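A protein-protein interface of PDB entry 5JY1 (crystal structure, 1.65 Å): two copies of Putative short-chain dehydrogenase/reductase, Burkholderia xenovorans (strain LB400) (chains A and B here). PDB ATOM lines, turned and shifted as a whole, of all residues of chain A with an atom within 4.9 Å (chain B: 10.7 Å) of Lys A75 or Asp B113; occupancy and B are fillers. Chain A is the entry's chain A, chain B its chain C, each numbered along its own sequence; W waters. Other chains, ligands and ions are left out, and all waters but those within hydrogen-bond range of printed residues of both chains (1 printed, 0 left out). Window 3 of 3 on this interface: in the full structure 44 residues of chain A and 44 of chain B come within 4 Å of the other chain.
Printed residues of chain B that touch a printed residue of chain A: Leu B108, Glu B109, Lys B111, Asp B113, Leu B116, Glu B117 and Leu B120.
Of the 11 printed residues of chain A, 5 touch a printed residue of chain B.
Hydrophobic or aromatic side chains of chain A within 4 Å of the printed part of chain B: Trp A125, Trp A128 and Trp A129.
Among the printed residues, 14 pairs touch across the chains.
Among the printed residues, Asp or Glu carboxylates within 4 Å of a Lys or Arg side-chain nitrogen of the other chain: Lys A75 with Asp B113 (3.0 Å) and Arg A132 with Asp B113 (3.6 Å).
Ser A74 touches none of the printed residues of chain B.
Of chain B, only Asp B113 (3.0 Å) comes within 4 Å of Lys A75.
No residue of chain B comes within 4 Å of Ala A76.
No residue of chain B comes within 4 Å of Ser A77.
No residue of chain B comes within 4 Å of Ile A78.
No residue of chain B comes within 4 Å of Glu A79.
Of chain B, only Asp B113 (3.0 Å) comes within 4 Å of Trp A129.
Printed residues of chain A within 4 Å of Glu B109: Arg A132.
Of the printed residues of chain A, Lys B111 touches Trp A128 and Arg A132.
Asp B113 touches just these residues of chain A: Lys A75, Trp A125, Trp A128, Trp A129 and Arg A132.
Of the printed residues of chain A, Glu B117 touches Trp A125.
Of the printed residues of chain A, Leu B120 touches Trp A125.
The nearest printed residue of chain A that does not touch Asp B113 is Glu A79 (7.0 Å).
The nearest printed residue of chain A that does not touch Glu B109 is Trp A128 (6.9 Å).
The backbone carbonyl oxygen (O) of Glu B117 lies within hydrogen-bond range of the side-chain hydroxyl (OG1) of Thr B121 (2.9 Å).
The side-chain amino group of Lys B111 sits at hydrogen-bond distance from the side-chain hydroxyl of Thr B103, 3.3 Å away.
The side-chain carboxylate (OD1) of Asp B163 is in salt-bridge range of the side-chain amino group (NZ) of Lys B111, at 2.9 Å.
The backbone carbonyl oxygen of Pro B104 lies within hydrogen-bond range of the side-chain amino group of Lys B111 (2.8 Å).
Trp A125 touches Asp B113.
Leu B116 touches Trp A125.
Trp A125 touches Glu B117 (CZ2 to OE1, 3.3 Å).
Leu B120 touches Trp A125.
Trp A128 touches Leu B108.
Lys B111 touches Trp A128.
Trp A128 touches Leu B116 (CD2 to CD2, 3.5 Å).
Glu B109 touches Arg A132 (O to NH1, 3.9 Å).
Water W1 bridges the backbone carbonyl oxygen of Glu B109 (2.9 Å) and the guanidinium group of Arg A132 (3.5 Å).
No position is printed for both chains.
NH2 of Arg A132 lies within salt-bridge range of OD1 of Asp B113 (3.6 Å).
OD1 of Asp B113 lies within hydrogen-bond range of NE1 of Trp A128, 2.9 Å away.
The backbone carbonyl oxygen (O) of Lys B111 sits at hydrogen-bond distance from the guanidinium group (NH1) of Arg A132 (2.7 Å).
The indole nitrogen (NE1) of Trp A129 is in hydrogen-bond range of the side-chain carboxylate (OD2) of Asp B113 (3.0 Å).
The side-chain carboxylate (OD2) of Asp B113 is in salt-bridge range of the side-chain amino group (NZ) of Lys A75 (3.0 Å).
The guanidinium group of Arg A132 lies within hydrogen-bond range of the backbone carbonyl oxygen of Leu B108.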
ATOM      1  N   THR A  73      13.939 -27.595  33.404  1.00  0.00           N
ATOM      2  CA  THR A  73      15.178 -27.873  32.683  1.00  0.00           C
ATOM      3  C   THR A  73      14.983 -27.848  31.172  1.00  0.00           C
ATOM      4  O   THR A  73      15.966 -27.988  30.433  1.00  0.00           O
ATOM      5  CB  THR A  73      15.773 -29.221  33.109  1.00  0.00           C
ATOM      6  OG1 THR A  73      14.920 -30.289  32.686  1.00  0.00           O
ATOM      7  CG2 THR A  73      15.953 -29.284  34.625  1.00  0.00           C
ATOM      8  N   SER A  74      13.751 -27.642  30.694  1.00  0.00           N
ATOM      9  CA  SER A  74      13.447 -27.626  29.268  1.00  0.00           C
ATOM     10  C   SER A  74      12.862 -26.277  28.891  1.00  0.00           C
ATOM     11  O   SER A  74      11.783 -25.907  29.365  1.00  0.00           O
ATOM     12  CB  SER A  74      12.473 -28.741  28.895  1.00  0.00           C
ATOM     13  OG  SER A  74      12.002 -28.542  27.569  1.00  0.00           O
ATOM     14  N   LYS A  75      13.571 -25.554  28.024  1.00  0.00           N
ATOM     15  CA  LYS A  75      13.083 -24.276  27.522  1.00  0.00           C
ATOM     16  C   LYS A  75      11.687 -24.409  26.915  1.00  0.00           C
ATOM     17  O   LYS A  75      10.806 -23.579  27.164  1.00  0.00           O
ATOM     18  CB  LYS A  75      14.073 -23.746  26.488  1.00  0.00           C
ATOM     19  CG  LYS A  75      13.689 -22.440  25.851  1.00  0.00           C
ATOM     20  CD  LYS A  75      14.692 -22.104  24.762  1.00  0.00           C
ATOM     21  CE  LYS A  75      14.562 -20.673  24.287  1.00  0.00           C
ATOM     22  NZ  LYS A  75      15.649 -20.381  23.306  1.00  0.00           N
ATOM     23  N   ALA A  76      11.469 -25.452  26.110  1.00  0.00           N
ATOM     24  CA  ALA A  76      10.166 -25.627  25.470  1.00  0.00           C
ATOM     25  C   ALA A  76       9.057 -25.802  26.500  1.00  0.00           C
ATOM     26  O   ALA A  76       7.957 -25.272  26.324  1.00  0.00           O
ATOM     27  CB  ALA A  76      10.198 -26.820  24.514  1.00  0.00           C
ATOM     28  N   SER A  77       9.329 -26.538  27.582  1.00  0.00           N
ATOM     29  CA  SER A  77       8.301 -26.787  28.592  1.00  0.00           C
ATOM     30  C   SER A  77       7.923 -25.505  29.320  1.00  0.00           C
ATOM     31  O   SER A  77       6.740 -25.253  29.582  1.00  0.00           O
ATOM     32  CB  SER A  77       8.796 -27.833  29.593  1.00  0.00           C
ATOM     33  OG  SER A  77       7.802 -28.123  30.570  1.00  0.00           O
ATOM     34  N   ILE A  78       8.922 -24.688  29.652  1.00  0.00           N
ATOM     35  CA  ILE A  78       8.667 -23.389  30.269  1.00  0.00           C
ATOM     36  C   ILE A  78       7.845 -22.510  29.334  1.00  0.00           C
ATOM     37  O   ILE A  78       6.863 -21.881  29.746  1.00  0.00           O
ATOM     38  CB  ILE A  78      10.000 -22.718  30.643  1.00  0.00           C
ATOM     39  CG1 ILE A  78      10.689 -23.487  31.766  1.00  0.00           C
ATOM     40  CG2 ILE A  78       9.756 -21.280  31.025  1.00  0.00           C
ATOM     41  CD1 ILE A  78      12.124 -23.026  32.030  1.00  0.00           C
ATOM     42  N   GLU A  79       8.243 -22.450  28.058  1.00  0.00           N
ATOM     43  CA  GLU A  79       7.528 -21.613  27.101  1.00  0.00           C
ATOM     44  C   GLU A  79       6.094 -22.091  26.928  1.00  0.00           C
ATOM     45  O   GLU A  79       5.166 -21.278  26.830  1.00  0.00           O
ATOM     46  CB  GLU A  79       8.265 -21.604  25.756  1.00  0.00           C
ATOM     47  CG  GLU A  79       9.565 -20.818  25.811  1.00  0.00           C
ATOM     48  CD  GLU A  79      10.313 -20.803  24.498  1.00  0.00           C
ATOM     49  OE1 GLU A  79      10.043 -21.672  23.651  1.00  0.00           O
ATOM     50  OE2 GLU A  79      11.183 -19.922  24.324  1.00  0.00           O
ATOM     51  N   TRP A 125      19.498 -21.309  34.281  1.00  0.00           N
ATOM     52  CA  TRP A 125      18.867 -21.392  32.967  1.00  0.00           C
ATOM     53  C   TRP A 125      17.347 -21.374  33.079  1.00  0.00           C
ATOM     54  O   TRP A 125      16.661 -20.704  32.292  1.00  0.00           O
ATOM     55  CB  TRP A 125      19.336 -22.652  32.246  1.00  0.00           C
ATOM     56  CG  TRP A 125      20.698 -22.495  31.625  1.00  0.00           C
ATOM     57  CD1 TRP A 125      21.892 -22.935  32.127  1.00  0.00           C
ATOM     58  CD2 TRP A 125      20.997 -21.842  30.388  1.00  0.00           C
ATOM     59  NE1 TRP A 125      22.923 -22.594  31.267  1.00  0.00           N
ATOM     60  CE2 TRP A 125      22.392 -21.930  30.191  1.00  0.00           C
ATOM     61  CE3 TRP A 125      20.212 -21.204  29.416  1.00  0.00           C
ATOM     62  CZ2 TRP A 125      23.023 -21.406  29.057  1.00  0.00           C
ATOM     63  CZ3 TRP A 125      20.835 -20.673  28.304  1.00  0.00           C
ATOM     64  CH2 TRP A 125      22.230 -20.783  28.127  1.00  0.00           C
ATOM     65  N   TRP A 128      16.385 -17.788  33.530  1.00  0.00           N
ATOM     66  CA  TRP A 128      16.616 -17.109  32.255  1.00  0.00           C
ATOM     67  C   TRP A 128      15.514 -17.402  31.239  1.00  0.00           C
ATOM     68  O   TRP A 128      14.954 -16.481  30.633  1.00  0.00           O
ATOM     69  CB  TRP A 128      17.985 -17.551  31.721  1.00  0.00           C
ATOM     70  CG  TRP A 128      18.391 -17.180  30.298  1.00  0.00           C
ATOM     71  CD1 TRP A 128      18.179 -17.914  29.169  1.00  0.00           C
ATOM     72  CD2 TRP A 128      19.177 -16.048  29.896  1.00  0.00           C
ATOM     73  NE1 TRP A 128      18.750 -17.292  28.081  1.00  0.00           N
ATOM     74  CE2 TRP A 128      19.372 -16.143  28.505  1.00  0.00           C
ATOM     75  CE3 TRP A 128      19.743 -14.966  30.582  1.00  0.00           C
ATOM     76  CZ2 TRP A 128      20.092 -15.190  27.784  1.00  0.00           C
ATOM     77  CZ3 TRP A 128      20.448 -14.021  29.865  1.00  0.00           C
ATOM     78  CH2 TRP A 128      20.618 -14.134  28.486  1.00  0.00           C
ATOM     79  N   TRP A 129      15.199 -18.686  31.030  1.00  0.00           N
ATOM     80  CA  TRP A 129      14.191 -19.051  30.037  1.00  0.00           C
ATOM     81  C   TRP A 129      12.817 -18.525  30.430  1.00  0.00           C
ATOM     82  O   TRP A 129      12.067 -18.022  29.585  1.00  0.00           O
ATOM     83  CB  TRP A 129      14.136 -20.569  29.880  1.00  0.00           C
ATOM     84  CG  TRP A 129      15.289 -21.163  29.145  1.00  0.00           C
ATOM     85  CD1 TRP A 129      15.956 -20.620  28.086  1.00  0.00           C
ATOM     86  CD2 TRP A 129      15.916 -22.421  29.419  1.00  0.00           C
ATOM     87  NE1 TRP A 129      16.963 -21.474  27.675  1.00  0.00           N
ATOM     88  CE2 TRP A 129      16.958 -22.584  28.480  1.00  0.00           C
ATOM     89  CE3 TRP A 129      15.701 -23.423  30.371  1.00  0.00           C
ATOM     90  CZ2 TRP A 129      17.778 -23.709  28.462  1.00  0.00           C
ATOM     91  CZ3 TRP A 129      16.520 -24.547  30.349  1.00  0.00           C
ATOM     92  CH2 TRP A 129      17.544 -24.677  29.400  1.00  0.00           C
ATOM     93  N   ARG A 132      12.579 -14.590  30.015  1.00  0.00           N
ATOM     94  CA  ARG A 132      12.453 -14.142  28.633  1.00  0.00           C
ATOM     95  C   ARG A 132      11.128 -14.570  27.997  1.00  0.00           C
ATOM     96  O   ARG A 132      10.608 -13.854  27.135  1.00  0.00           O
ATOM     97  CB  ARG A 132      13.658 -14.630  27.825  1.00  0.00           C
ATOM     98  CG  ARG A 132      14.935 -13.850  28.199  1.00  0.00           C
ATOM     99  CD  ARG A 132      16.220 -14.700  28.163  1.00  0.00           C
ATOM    100  NE  ARG A 132      16.423 -15.407  26.894  1.00  0.00           N
ATOM    101  CZ  ARG A 132      17.017 -14.884  25.824  1.00  0.00           C
ATOM    102  NH1 ARG A 132      17.448 -13.630  25.836  1.00  0.00           N
ATOM    103  NH2 ARG A 132      17.188 -15.621  24.731  1.00  0.00           N
ATOM    104  N   THR B 103      30.555 -10.808  23.922  1.00  0.00           N
ATOM    105  CA  THR B 103      29.389 -11.088  23.097  1.00  0.00           C
ATOM    106  C   THR B 103      28.767  -9.766  22.643  1.00  0.00           C
ATOM    107  O   THR B 103      29.044  -8.711  23.230  1.00  0.00           O
ATOM    108  CB  THR B 103      28.343 -11.916  23.863  1.00  0.00           C
ATOM    109  OG1 THR B 103      27.922 -11.188  25.030  1.00  0.00           O
ATOM    110  CG2 THR B 103      28.931 -13.258  24.290  1.00  0.00           C
ATOM    111  N   PRO B 104      27.936  -9.779  21.596  1.00  0.00           N
ATOM    112  CA  PRO B 104      27.384  -8.517  21.083  1.00  0.00           C
ATOM    113  C   PRO B 104      26.636  -7.740  22.158  1.00  0.00           C
ATOM    114  O   PRO B 104      25.927  -8.312  22.987  1.00  0.00           O
ATOM    115  CB  PRO B 104      26.443  -8.975  19.963  1.00  0.00           C
ATOM    116  CG  PRO B 104      27.084 -10.239  19.463  1.00  0.00           C
ATOM    117  CD  PRO B 104      27.580 -10.912  20.715  1.00  0.00           C
ATOM    118  N   VAL B 106      23.773  -6.186  23.059  1.00  0.00           N
ATOM    119  CA  VAL B 106      22.381  -6.163  22.630  1.00  0.00           C
ATOM    120  C   VAL B 106      21.514  -6.244  23.880  1.00  0.00           C
ATOM    121  O   VAL B 106      21.965  -6.669  24.949  1.00  0.00           O
ATOM    122  CB  VAL B 106      22.037  -7.308  21.639  1.00  0.00           C
ATOM    123  CG1 VAL B 106      22.850  -7.166  20.347  1.00  0.00           C
ATOM    124  CG2 VAL B 106      22.274  -8.671  22.274  1.00  0.00           C
ATOM    125  N   LEU B 107      20.262  -5.802  23.738  1.00  0.00           N
ATOM    126  CA  LEU B 107      19.337  -5.798  24.866  1.00  0.00           C
ATOM    127  C   LEU B 107      19.088  -7.230  25.331  1.00  0.00           C
ATOM    128  O   LEU B 107      19.278  -8.194  24.586  1.00  0.00           O
ATOM    129  CB  LEU B 107      18.027  -5.107  24.467  1.00  0.00           C
ATOM    130  CG  LEU B 107      18.199  -3.597  24.236  1.00  0.00           C
ATOM    131  CD1 LEU B 107      16.986  -2.987  23.560  1.00  0.00           C
ATOM    132  CD2 LEU B 107      18.475  -2.876  25.550  1.00  0.00           C
ATOM    133  N   LEU B 108      18.697  -7.364  26.599  1.00  0.00           N
ATOM    134  CA  LEU B 108      18.612  -8.687  27.223  1.00  0.00           C
ATOM    135  C   LEU B 108      17.725  -9.641  26.429  1.00  0.00           C
ATOM    136  O   LEU B 108      18.092 -10.807  26.220  1.00  0.00           O
ATOM    137  CB  LEU B 108      18.099  -8.543  28.663  1.00  0.00           C
ATOM    138  CG  LEU B 108      17.943  -9.802  29.519  1.00  0.00           C
ATOM    139  CD1 LEU B 108      19.255 -10.551  29.650  1.00  0.00           C
ATOM    140  CD2 LEU B 108      17.452  -9.378  30.905  1.00  0.00           C
ATOM    141  N   GLU B 109      16.567  -9.165  25.958  1.00  0.00           N
ATOM    142  CA  GLU B 109      15.668 -10.025  25.193  1.00  0.00           C
ATOM    143  C   GLU B 109      16.233 -10.389  23.827  1.00  0.00           C
ATOM    144  O   GLU B 109      15.704 -11.303  23.182  1.00  0.00           O
ATOM    145  CB  GLU B 109      14.284  -9.363  25.038  1.00  0.00           C
ATOM    146  CG  GLU B 109      14.268  -8.076  24.215  1.00  0.00           C
ATOM    147  CD  GLU B 109      14.510  -6.813  25.039  1.00  0.00           C
ATOM    148  OE1 GLU B 109      14.147  -5.709  24.568  1.00  0.00           O
ATOM    149  OE2 GLU B 109      15.068  -6.918  26.147  1.00  0.00           O
ATOM    150  N   GLU B 110      17.289  -9.707  23.376  1.00  0.00           N
ATOM    151  CA  GLU B 110      17.943 -10.049  22.115  1.00  0.00           C
ATOM    152  C   GLU B 110      19.129 -10.981  22.289  1.00  0.00           C
ATOM    153  O   GLU B 110      19.578 -11.572  21.296  1.00  0.00           O
ATOM    154  CB  GLU B 110      18.429  -8.784  21.397  1.00  0.00           C
ATOM    155  CG  GLU B 110      17.345  -7.754  21.110  1.00  0.00           C
ATOM    156  CD  GLU B 110      16.254  -8.251  20.171  1.00  0.00           C
ATOM    157  OE1 GLU B 110      16.539  -9.081  19.279  1.00  0.00           O
ATOM    158  OE2 GLU B 110      15.103  -7.804  20.332  1.00  0.00           O
ATOM    159  N   LYS B 111      19.683 -11.088  23.502  1.00  0.00           N
ATOM    160  CA  LYS B 111      20.740 -12.063  23.739  1.00  0.00           C
ATOM    161  C   LYS B 111      20.235 -13.459  23.387  1.00  0.00           C
ATOM    162  O   LYS B 111      19.073 -13.792  23.629  1.00  0.00           O
ATOM    163  CB  LYS B 111      21.186 -12.021  25.207  1.00  0.00           C
ATOM    164  CG  LYS B 111      21.800 -10.689  25.669  1.00  0.00           C
ATOM    165  CD  LYS B 111      23.296 -10.617  25.318  1.00  0.00           C
ATOM    166  CE  LYS B 111      23.898  -9.297  25.794  1.00  0.00           C
ATOM    167  NZ  LYS B 111      25.371  -9.181  25.583  1.00  0.00           N
ATOM    168  N   THR B 112      21.100 -14.268  22.782  1.00  0.00           N
ATOM    169  CA  THR B 112      20.748 -15.651  22.504  1.00  0.00           C
ATOM    170  C   THR B 112      21.235 -16.568  23.624  1.00  0.00           C
ATOM    171  O   THR B 112      22.135 -16.222  24.394  1.00  0.00           O
ATOM    172  CB  THR B 112      21.360 -16.110  21.182  1.00  0.00           C
ATOM    173  OG1 THR B 112      22.793 -16.078  21.301  1.00  0.00           O
ATOM    174  CG2 THR B 112      20.911 -15.191  20.050  1.00  0.00           C
ATOM    175  N   ASP B 113      20.625 -17.758  23.701  1.00  0.00           N
ATOM    176  CA  ASP B 113      21.117 -18.774  24.628  1.00  0.00           C
ATOM    177  C   ASP B 113      22.581 -19.096  24.357  1.00  0.00           C
ATOM    178  O   ASP B 113      23.353 -19.363  25.285  1.00  0.00           O
ATOM    179  CB  ASP B 113      20.276 -20.051  24.528  1.00  0.00           C
ATOM    180  CG  ASP B 113      18.877 -19.887  25.103  1.00  0.00           C
ATOM    181  OD1 ASP B 113      18.548 -18.808  25.643  1.00  0.00           O
ATOM    182  OD2 ASP B 113      18.101 -20.862  25.009  1.00  0.00           O
ATOM    183  N   GLU B 114      22.977 -19.081  23.083  1.00  0.00           N
ATOM    184  CA  GLU B 114      24.362 -19.372  22.726  1.00  0.00           C
ATOM    185  C   GLU B 114      25.316 -18.350  23.334  1.00  0.00           C
ATOM    186  O   GLU B 114      26.434 -18.694  23.746  1.00  0.00           O
ATOM    187  CB  GLU B 114      24.503 -19.402  21.205  1.00  0.00           C
ATOM    188  CG  GLU B 114      23.861 -20.622  20.534  1.00  0.00           C
ATOM    189  CD  GLU B 114      22.342 -20.675  20.686  1.00  0.00           C
ATOM    190  OE1 GLU B 114      21.684 -19.608  20.657  1.00  0.00           O
ATOM    191  OE2 GLU B 114      21.809 -21.795  20.844  1.00  0.00           O
ATOM    192  N   MET B 115      24.890 -17.085  23.402  1.00  0.00           N
ATOM    193  CA  MET B 115      25.721 -16.064  24.035  1.00  0.00           C
ATOM    194  C   MET B 115      25.890 -16.333  25.523  1.00  0.00           C
ATOM    195  O   MET B 115      26.994 -16.208  26.061  1.00  0.00           O
ATOM    196  CB  MET B 115      25.116 -14.679  23.824  1.00  0.00           C
ATOM    197  CG  MET B 115      25.196 -14.208  22.386  1.00  0.00           C
ATOM    198  SD  MET B 115      24.268 -12.684  22.136  1.00  0.00           S
ATOM    199  CE  MET B 115      24.126 -12.649  20.352  1.00  0.00           C
ATOM    200  N   LEU B 116      24.798 -16.664  26.217  1.00  0.00           N
ATOM    201  CA  LEU B 116      24.912 -16.946  27.643  1.00  0.00           C
ATOM    202  C   LEU B 116      25.776 -18.176  27.887  1.00  0.00           C
ATOM    203  O   LEU B 116      26.619 -18.174  28.787  1.00  0.00           O
ATOM    204  CB  LEU B 116      23.525 -17.111  28.278  1.00  0.00           C
ATOM    205  CG  LEU B 116      23.569 -17.459  29.774  1.00  0.00           C
ATOM    206  CD1 LEU B 116      24.227 -16.345  30.610  1.00  0.00           C
ATOM    207  CD2 LEU B 116      22.168 -17.774  30.308  1.00  0.00           C
ATOM    208  N   GLU B 117      25.621 -19.215  27.065  1.00  0.00           N
ATOM    209  CA  GLU B 117      26.442 -20.410  27.243  1.00  0.00           C
ATOM    210  C   GLU B 117      27.914 -20.099  27.010  1.00  0.00           C
ATOM    211  O   GLU B 117      28.784 -20.547  27.773  1.00  0.00           O
ATOM    212  CB  GLU B 117      25.971 -21.527  26.304  1.00  0.00           C
ATOM    213  CG  GLU B 117      26.711 -22.844  26.547  1.00  0.00           C
ATOM    214  CD  GLU B 117      26.763 -23.227  28.028  1.00  0.00           C
ATOM    215  OE1 GLU B 117      25.701 -23.249  28.690  1.00  0.00           O
ATOM    216  OE2 GLU B 117      27.873 -23.497  28.537  1.00  0.00           O
ATOM    217  N   GLN B 118      28.213 -19.307  25.978  1.00  0.00           N
ATOM    218  CA  GLN B 118      29.603 -18.952  25.707  1.00  0.00           C
ATOM    219  C   GLN B 118      30.202 -18.151  26.856  1.00  0.00           C
ATOM    220  O   GLN B 118      31.342 -18.398  27.274  1.00  0.00           O
ATOM    221  CB  GLN B 118      29.696 -18.158  24.407  1.00  0.00           C
ATOM    222  CG  GLN B 118      31.127 -17.792  24.028  1.00  0.00           C
ATOM    223  CD  GLN B 118      31.186 -16.852  22.845  1.00  0.00           C
ATOM    224  OE1 GLN B 118      31.468 -15.660  22.996  1.00  0.00           O
ATOM    225  NE2 GLN B 118      30.921 -17.383  21.659  1.00  0.00           N
ATOM    226  N   THR B 119      29.442 -17.191  27.381  1.00  0.00           N
ATOM    227  CA  THR B 119      29.935 -16.353  28.470  1.00  0.00           C
ATOM    228  C   THR B 119      30.073 -17.142  29.768  1.00  0.00           C
ATOM    229  O   THR B 119      31.056 -16.970  30.500  1.00  0.00           O
ATOM    230  CB  THR B 119      29.015 -15.147  28.648  1.00  0.00           C
ATOM    231  OG1 THR B 119      29.123 -14.310  27.493  1.00  0.00           O
ATOM    232  CG2 THR B 119      29.425 -14.334  29.867  1.00  0.00           C
ATOM    233  N   LEU B 120      29.112 -18.019  30.070  1.00  0.00           N
ATOM    234  CA  LEU B 120      29.276 -18.909  31.220  1.00  0.00           C
ATOM    235  C   LEU B 120      30.528 -19.774  31.090  1.00  0.00           C
ATOM    236  O   LEU B 120      31.222 -20.026  32.078  1.00  0.00           O
ATOM    237  CB  LEU B 120      28.039 -19.795  31.382  1.00  0.00           C
ATOM    238  CG  LEU B 120      26.796 -19.104  31.936  1.00  0.00           C
ATOM    239  CD1 LEU B 120      25.590 -20.026  31.864  1.00  0.00           C
ATOM    240  CD2 LEU B 120      27.049 -18.650  33.378  1.00  0.00           C
ATOM    241  N   THR B 121      30.834 -20.239  29.880  1.00  0.00           N
ATOM    242  CA  THR B 121      32.003 -21.096  29.695  1.00  0.00           C
ATOM    243  C   THR B 121      33.296 -20.310  29.882  1.00  0.00           C
ATOM    244  O   THR B 121      34.202 -20.748  30.605  1.00  0.00           O
ATOM    245  CB  THR B 121      31.974 -21.744  28.312  1.00  0.00           C
ATOM    246  OG1 THR B 121      30.834 -22.606  28.200  1.00  0.00           O
ATOM    247  CG2 THR B 121      33.248 -22.567  28.097  1.00  0.00           C
ATOM    248  N   GLY B 162      23.777  -8.368  29.769  1.00  0.00           N
ATOM    249  CA  GLY B 162      23.033  -9.276  30.637  1.00  0.00           C
ATOM    250  C   GLY B 162      23.711 -10.621  30.868  1.00  0.00           C
ATOM    251  O   GLY B 162      23.713 -11.141  31.983  1.00  0.00           O
ATOM    252  N   ASP B 163      24.277 -11.219  29.813  1.00  0.00           N
ATOM    253  CA  ASP B 163      24.926 -12.515  30.004  1.00  0.00           C
ATOM    254  C   ASP B 163      26.207 -12.373  30.817  1.00  0.00           C
ATOM    255  O   ASP B 163      26.483 -13.180  31.713  1.00  0.00           O
ATOM    256  CB  ASP B 163      25.203 -13.179  28.640  1.00  0.00           C
ATOM    257  CG  ASP B 163      25.968 -12.274  27.664  1.00  0.00           C
ATOM    258  OD1 ASP B 163      25.841 -11.030  27.705  1.00  0.00           O
ATOM    259  OD2 ASP B 163      26.693 -12.831  26.813  1.00  0.00           O
ATOM    260  N   TYR B 164      26.990 -11.343  30.523  1.00  0.00           N
ATOM    261  CA  TYR B 164      28.208 -11.063  31.273  1.00  0.00           C
ATOM    262  C   TYR B 164      27.905 -10.797  32.749  1.00  0.00           C
ATOM    263  O   TYR B 164      28.565 -11.351  33.641  1.00  0.00           O
ATOM    264  CB  TYR B 164      28.887  -9.877  30.588  1.00  0.00           C
ATOM    265  CG  TYR B 164      30.099  -9.290  31.226  1.00  0.00           C
ATOM    266  CD1 TYR B 164      31.362  -9.820  30.978  1.00  0.00           C
ATOM    267  CD2 TYR B 164      30.007  -8.144  31.998  1.00  0.00           C
ATOM    268  CE1 TYR B 164      32.494  -9.256  31.534  1.00  0.00           C
ATOM    269  CE2 TYR B 164      31.132  -7.570  32.560  1.00  0.00           C
ATOM    270  CZ  TYR B 164      32.370  -8.128  32.323  1.00  0.00           C
ATOM    271  OH  TYR B 164      33.488  -7.556  32.876  1.00  0.00           O
ATOM    272  N   THR B 166      25.470 -11.829  34.521  1.00  0.00           N
ATOM    273  CA  THR B 166      25.043 -13.069  35.157  1.00  0.00           C
ATOM    274  C   THR B 166      26.238 -13.954  35.481  1.00  0.00           C
ATOM    275  O   THR B 166      26.389 -14.416  36.617  1.00  0.00           O
ATOM    276  CB  THR B 166      24.053 -13.795  34.235  1.00  0.00           C
ATOM    277  OG1 THR B 166      22.896 -12.961  34.033  1.00  0.00           O
ATOM    278  CG2 THR B 166      23.611 -15.127  34.840  1.00  0.00           C
HETATM  279  O   HOH W   1      14.225 -13.318  24.573  1.00  0.00           O
